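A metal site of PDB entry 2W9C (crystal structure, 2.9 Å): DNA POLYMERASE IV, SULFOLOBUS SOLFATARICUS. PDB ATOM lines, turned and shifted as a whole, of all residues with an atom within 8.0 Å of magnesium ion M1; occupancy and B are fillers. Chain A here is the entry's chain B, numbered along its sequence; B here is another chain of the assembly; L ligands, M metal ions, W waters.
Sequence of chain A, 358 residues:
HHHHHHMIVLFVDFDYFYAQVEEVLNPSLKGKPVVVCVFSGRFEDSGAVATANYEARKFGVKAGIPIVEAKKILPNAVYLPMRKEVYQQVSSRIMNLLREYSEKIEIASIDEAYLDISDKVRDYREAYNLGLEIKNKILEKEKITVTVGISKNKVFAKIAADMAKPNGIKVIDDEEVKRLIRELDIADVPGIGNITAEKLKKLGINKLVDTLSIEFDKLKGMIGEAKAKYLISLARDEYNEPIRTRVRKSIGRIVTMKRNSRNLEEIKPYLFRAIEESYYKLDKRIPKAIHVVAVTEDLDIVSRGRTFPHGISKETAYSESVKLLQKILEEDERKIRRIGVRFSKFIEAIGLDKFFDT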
ATOM      1  N   PHE A  11     -20.299 -26.654  14.613  1.00  0.00           N
ATOM      2  CA  PHE A  11     -20.612 -25.328  14.061  1.00  0.00           C
ATOM      3  C   PHE A  11     -21.606 -25.389  12.884  1.00  0.00           C
ATOM      4  O   PHE A  11     -21.380 -26.100  11.898  1.00  0.00           O
ATOM      5  CB  PHE A  11     -19.293 -24.654  13.628  1.00  0.00           C
ATOM      6  CG  PHE A  11     -19.456 -23.309  13.000  1.00  0.00           C
ATOM      7  CD1 PHE A  11     -19.878 -22.219  13.750  1.00  0.00           C
ATOM      8  CD2 PHE A  11     -19.194 -23.121  11.643  1.00  0.00           C
ATOM      9  CE1 PHE A  11     -20.027 -20.947  13.150  1.00  0.00           C
ATOM     10  CE2 PHE A  11     -19.341 -21.854  11.035  1.00  0.00           C
ATOM     11  CZ  PHE A  11     -19.762 -20.777  11.803  1.00  0.00           C
ATOM     12  N   VAL A  12     -22.688 -24.630  12.979  1.00  0.00           N
ATOM     13  CA  VAL A  12     -23.669 -24.584  11.911  1.00  0.00           C
ATOM     14  C   VAL A  12     -23.582 -23.223  11.231  1.00  0.00           C
ATOM     15  O   VAL A  12     -23.535 -22.177  11.875  1.00  0.00           O
ATOM     16  CB  VAL A  12     -25.090 -24.801  12.458  1.00  0.00           C
ATOM     17  CG1 VAL A  12     -26.097 -24.869  11.315  1.00  0.00           C
ATOM     18  CG2 VAL A  12     -25.131 -26.074  13.265  1.00  0.00           C
ATOM     19  N   ASP A  13     -23.581 -23.252   9.898  1.00  0.00           N
ATOM     20  CA  ASP A  13     -23.444 -22.039   9.098  1.00  0.00           C
ATOM     21  C   ASP A  13     -24.575 -21.866   8.080  1.00  0.00           C
ATOM     22  O   ASP A  13     -24.501 -22.463   7.013  1.00  0.00           O
ATOM     23  CB  ASP A  13     -22.096 -22.129   8.390  1.00  0.00           C
ATOM     24  CG  ASP A  13     -21.490 -20.808   8.128  1.00  0.00           C
ATOM     25  OD1 ASP A  13     -21.083 -20.128   9.086  1.00  0.00           O
ATOM     26  OD2 ASP A  13     -21.415 -20.443   6.948  1.00  0.00           O
ATOM     27  N   PHE A  14     -25.598 -21.073   8.389  1.00  0.00           N
ATOM     28  CA  PHE A  14     -26.742 -20.849   7.468  1.00  0.00           C
ATOM     29  C   PHE A  14     -26.382 -20.412   6.011  1.00  0.00           C
ATOM     30  O   PHE A  14     -26.480 -19.235   5.688  1.00  0.00           O
ATOM     31  CB  PHE A  14     -27.675 -19.779   8.027  1.00  0.00           C
ATOM     32  CG  PHE A  14     -28.319 -20.118   9.333  1.00  0.00           C
ATOM     33  CD1 PHE A  14     -27.956 -21.257  10.044  1.00  0.00           C
ATOM     34  CD2 PHE A  14     -29.290 -19.265   9.865  1.00  0.00           C
ATOM     35  CE1 PHE A  14     -28.546 -21.530  11.284  1.00  0.00           C
ATOM     36  CE2 PHE A  14     -29.879 -19.533  11.091  1.00  0.00           C
ATOM     37  CZ  PHE A  14     -29.507 -20.670  11.804  1.00  0.00           C
ATOM     38  N   PHE A  17     -27.206 -16.885   3.865  1.00  0.00           N
ATOM     39  CA  PHE A  17     -28.403 -16.538   4.617  1.00  0.00           C
ATOM     40  C   PHE A  17     -29.474 -15.589   4.060  1.00  0.00           C
ATOM     41  O   PHE A  17     -30.609 -16.022   3.857  1.00  0.00           O
ATOM     42  CB  PHE A  17     -28.019 -16.072   6.018  1.00  0.00           C
ATOM     43  CG  PHE A  17     -29.177 -16.086   6.983  1.00  0.00           C
ATOM     44  CD1 PHE A  17     -30.160 -17.079   6.889  1.00  0.00           C
ATOM     45  CD2 PHE A  17     -29.255 -15.138   8.000  1.00  0.00           C
ATOM     46  CE1 PHE A  17     -31.210 -17.120   7.791  1.00  0.00           C
ATOM     47  CE2 PHE A  17     -30.298 -15.172   8.911  1.00  0.00           C
ATOM     48  CZ  PHE A  17     -31.279 -16.169   8.808  1.00  0.00           C
ATOM     49  N   TYR A  18     -29.119 -14.317   3.831  1.00  0.00           N
ATOM     50  CA  TYR A  18     -30.078 -13.331   3.306  1.00  0.00           C
ATOM     51  C   TYR A  18     -30.683 -13.774   1.977  1.00  0.00           C
ATOM     52  O   TYR A  18     -31.877 -13.702   1.771  1.00  0.00           O
ATOM     53  CB  TYR A  18     -29.385 -11.974   3.104  1.00  0.00           C
ATOM     54  CG  TYR A  18     -28.902 -11.295   4.377  1.00  0.00           C
ATOM     55  CD1 TYR A  18     -28.984 -11.921   5.629  1.00  0.00           C
ATOM     56  CD2 TYR A  18     -28.344 -10.007   4.325  1.00  0.00           C
ATOM     57  CE1 TYR A  18     -28.536 -11.295   6.772  1.00  0.00           C
ATOM     58  CE2 TYR A  18     -27.895  -9.381   5.468  1.00  0.00           C
ATOM     59  CZ  TYR A  18     -28.000 -10.027   6.691  1.00  0.00           C
ATOM     60  OH  TYR A  18     -27.531  -9.388   7.809  1.00  0.00           O
ATOM     61  N   MET A  95     -32.257 -20.899  15.443  1.00  0.00           N
ATOM     62  CA  MET A  95     -31.295 -20.967  16.540  1.00  0.00           C
ATOM     63  C   MET A  95     -31.949 -21.773  17.643  1.00  0.00           C
ATOM     64  O   MET A  95     -31.506 -22.878  17.967  1.00  0.00           O
ATOM     65  CB  MET A  95     -30.956 -19.580  17.084  1.00  0.00           C
ATOM     66  CG  MET A  95     -30.131 -18.710  16.150  1.00  0.00           C
ATOM     67  SD  MET A  95     -28.565 -19.479  15.753  1.00  0.00           S
ATOM     68  CE  MET A  95     -28.008 -18.469  14.355  1.00  0.00           C
ATOM     69  N   ALA A 108     -22.920 -16.832  17.790  1.00  0.00           N
ATOM     70  CA  ALA A 108     -22.024 -15.715  17.504  1.00  0.00           C
ATOM     71  C   ALA A 108     -22.486 -14.724  16.444  1.00  0.00           C
ATOM     72  O   ALA A 108     -22.003 -13.605  16.402  1.00  0.00           O
ATOM     73  CB  ALA A 108     -20.635 -16.240  17.149  1.00  0.00           C
ATOM     74  N   SER A 109     -23.410 -15.150  15.591  1.00  0.00           N
ATOM     75  CA  SER A 109     -23.935 -14.280  14.518  1.00  0.00           C
ATOM     76  C   SER A 109     -25.240 -14.815  13.948  1.00  0.00           C
ATOM     77  O   SER A 109     -25.555 -15.997  14.096  1.00  0.00           O
ATOM     78  CB  SER A 109     -22.912 -14.146  13.393  1.00  0.00           C
ATOM     79  OG  SER A 109     -23.492 -13.534  12.264  1.00  0.00           O
ATOM     80  N   ILE A 110     -25.984 -13.929  13.295  1.00  0.00           N
ATOM     81  CA  ILE A 110     -27.289 -14.231  12.689  1.00  0.00           C
ATOM     82  C   ILE A 110     -27.338 -15.521  11.869  1.00  0.00           C
ATOM     83  O   ILE A 110     -28.391 -16.159  11.730  1.00  0.00           O
ATOM     84  CB  ILE A 110     -27.768 -13.036  11.797  1.00  0.00           C
ATOM     85  CG1 ILE A 110     -29.267 -13.134  11.546  1.00  0.00           C
ATOM     86  CG2 ILE A 110     -27.073 -13.059  10.444  1.00  0.00           C
ATOM     87  CD1 ILE A 110     -29.862 -11.831  11.064  1.00  0.00           C
ATOM     88  N   ASP A 111     -26.189 -15.918  11.358  1.00  0.00           N
ATOM     89  CA  ASP A 111     -26.099 -17.084  10.510  1.00  0.00           C
ATOM     90  C   ASP A 111     -25.115 -18.101  11.057  1.00  0.00           C
ATOM     91  O   ASP A 111     -24.696 -19.020  10.346  1.00  0.00           O
ATOM     92  CB  ASP A 111     -25.633 -16.628   9.160  1.00  0.00           C
ATOM     93  CG  ASP A 111     -24.435 -15.718   9.266  1.00  0.00           C
ATOM     94  OD1 ASP A 111     -24.029 -15.128   8.247  1.00  0.00           O
ATOM     95  OD2 ASP A 111     -23.903 -15.597  10.384  1.00  0.00           O
ATOM     96  N   GLU A 112     -24.719 -17.916  12.315  1.00  0.00           N
ATOM     97  CA  GLU A 112     -23.761 -18.821  12.949  1.00  0.00           C
ATOM     98  C   GLU A 112     -23.944 -19.010  14.427  1.00  0.00           C
ATOM     99  O   GLU A 112     -24.339 -18.098  15.135  1.00  0.00           O
ATOM    100  CB  GLU A 112     -22.332 -18.313  12.705  1.00  0.00           C
ATOM    101  CG  GLU A 112     -22.009 -18.151  11.239  1.00  0.00           C
ATOM    102  CD  GLU A 112     -20.989 -17.063  11.009  1.00  0.00           C
ATOM    103  OE1 GLU A 112     -21.277 -15.911  11.383  1.00  0.00           O
ATOM    104  OE2 GLU A 112     -19.915 -17.382  10.453  1.00  0.00           O
ATOM    105  N   ALA A 113     -23.615 -20.220  14.868  1.00  0.00           N
ATOM    106  CA  ALA A 113     -23.707 -20.619  16.267  1.00  0.00           C
ATOM    107  C   ALA A 113     -22.990 -21.948  16.471  1.00  0.00           C
ATOM    108  O   ALA A 113     -23.215 -22.886  15.720  1.00  0.00           O
ATOM    109  CB  ALA A 113     -25.161 -20.724  16.693  1.00  0.00           C
ATOM    110  N   LYS A 158     -15.201 -24.354  12.649  1.00  0.00           N
ATOM    111  CA  LYS A 158     -15.586 -23.337  11.675  1.00  0.00           C
ATOM    112  C   LYS A 158     -14.973 -23.719  10.343  1.00  0.00           C
ATOM    113  O   LYS A 158     -15.685 -23.934   9.366  1.00  0.00           O
ATOM    114  CB  LYS A 158     -15.040 -21.983  12.112  1.00  0.00           C
ATOM    115  CG  LYS A 158     -15.095 -20.882  11.060  1.00  0.00           C
ATOM    116  CD  LYS A 158     -16.432 -20.209  11.034  1.00  0.00           C
ATOM    117  CE  LYS A 158     -16.434 -19.033  10.083  1.00  0.00           C
ATOM    118  NZ  LYS A 158     -17.829 -18.503   9.875  1.00  0.00           N
ATOM    119  N1  DOC B  13     -16.856  -8.966   6.933  1.00  0.00           N
ATOM    120  C2  DOC B  13     -17.899  -8.045   6.888  1.00  0.00           C
ATOM    121  N3  DOC B  13     -17.678  -6.808   6.382  1.00  0.00           N
ATOM    122  C4  DOC B  13     -16.458  -6.464   5.965  1.00  0.00           C
ATOM    123  C5  DOC B  13     -15.350  -7.354   6.089  1.00  0.00           C
ATOM    124  C6  DOC B  13     -15.586  -8.591   6.557  1.00  0.00           C
ATOM    125  O2  DOC B  13     -19.032  -8.396   7.285  1.00  0.00           O
ATOM    126  N4  DOC B  13     -16.293  -5.246   5.443  1.00  0.00           N
ATOM    127  C1' DOC B  13     -17.075 -10.301   7.363  1.00  0.00           C
ATOM    128  C2' DOC B  13     -16.553 -11.414   6.431  1.00  0.00           C
ATOM    129  C3' DOC B  13     -16.608 -12.730   7.439  1.00  0.00           C
ATOM    130  C4' DOC B  13     -16.276 -11.789   8.671  1.00  0.00           C
ATOM    131  O4' DOC B  13     -16.667 -10.622   8.660  1.00  0.00           O
ATOM    132  C5' DOC B  13     -15.087 -12.619   9.391  1.00  0.00           C
ATOM    133  O5' DOC B  13     -13.942 -12.151   8.483  1.00  0.00           O
ATOM    134  P   DOC B  13     -12.511 -12.837   8.880  1.00  0.00           P
ATOM    135  OP1 DOC B  13     -12.628 -14.195   9.448  1.00  0.00           O
ATOM    136  OP2 DOC B  13     -11.577 -12.623   7.739  1.00  0.00           O
HETATM  137  P1  LIG L   1     -19.184 -15.541   4.638  1.00  0.00           P
HETATM  138  O1  LIG L   1     -18.933 -16.541   5.836  1.00  0.00           O
HETATM  139  O2  LIG L   1     -17.956 -14.885   4.136  1.00  0.00           O
HETATM  140  O3  LIG L   1     -19.955 -16.376   3.488  1.00  0.00           O
HETATM  141  P2  LIG L   1     -21.161 -17.340   3.989  1.00  0.00           P
HETATM  142  O4  LIG L   1     -20.965 -17.477   5.567  1.00  0.00           O
HETATM  143  O5  LIG L   1     -21.232 -18.641   3.284  1.00  0.00           O
HETATM  144  O6  LIG L   1     -22.491 -16.453   3.825  1.00  0.00           O
HETATM  145  P3  LIG L   1     -23.173 -15.972   5.193  1.00  0.00           P
HETATM  146  O7  LIG L   1     -22.014 -16.149   6.323  1.00  0.00           O
HETATM  147  O8  LIG L   1     -24.280 -17.087   5.507  1.00  0.00           O
HETATM  148  O9  LIG L   1     -23.721 -14.604   5.135  1.00  0.00           O
HETATM  149  O10 LIG L   1     -20.286 -14.493   5.190  1.00  0.00           O
HETATM  150  C1  LIG L   1     -19.859 -13.212   5.636  1.00  0.00           C
HETATM  151  C2  LIG L   1     -20.943 -12.172   5.271  1.00  0.00           C
HETATM  152  O11 LIG L   1     -20.425 -10.884   5.553  1.00  0.00           O
HETATM  153  C3  LIG L   1     -21.216 -12.234   3.775  1.00  0.00           C
HETATM  154  O12 LIG L   1     -22.455 -12.909   3.542  1.00  0.00           O
HETATM  155  C4  LIG L   1     -21.445 -10.778   3.395  1.00  0.00           C
HETATM  156  C5  LIG L   1     -21.060  -9.976   4.629  1.00  0.00           C
HETATM  157  N1  LIG L   1     -19.971  -9.103   4.169  1.00  0.00           N
HETATM  158  C6  LIG L   1     -20.270  -7.766   3.911  1.00  0.00           C
HETATM  159  O13 LIG L   1     -21.373  -7.314   4.188  1.00  0.00           O
HETATM  160  N2  LIG L   1     -19.290  -6.969   3.302  1.00  0.00           N
HETATM  161  C7  LIG L   1     -18.055  -7.548   2.960  1.00  0.00           C
HETATM  162  O14 LIG L   1     -17.210  -6.819   2.398  1.00  0.00           O
HETATM  163  C8  LIG L   1     -17.771  -8.866   3.215  1.00  0.00           C
HETATM  164  C9  LIG L   1     -16.435  -9.484   2.790  1.00  0.00           C
HETATM  165  C10 LIG L   1     -18.732  -9.663   3.840  1.00  0.00           C
HETATM  166 MG    MG M   1     -22.271 -14.516  10.497  1.00  0.00          MG
HETATM  167 MG    MG M   2     -22.516 -18.192   6.810  1.00  0.00          MG
HETATM  168  O   HOH W   1     -22.607 -12.531   9.086  1.00  0.00           O
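N3 of DOC 13 of chain B sits at hydrogen-bond distance from N2 of the ligand, at 3.5 Å. N of Phe 17 lies close to O8 of the ligand, at 3.4 Å.
The backbone NH of Phe 14 is in hydrogen-bond range of the backbone carbonyl oxygen of Asp 111 (3.0 Å). OE2 of Glu 112 lies within salt-bridge range of NZ of Lys 158, 2.4 Å away.
Of the 15 residues printed, 3 come within 4 Å of magnesium ion M1. The nearest printed residue that does not touch magnesium ion M1 is Ile 110 (4.7 Å).
Magnesium ion M1 is bound by OE1 of Glu 112 (1.9 Å), OD2 of Asp 111 (2.0 Å), OG of Ser 109 (2.4 Å) and water W1 (2.5 Å).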
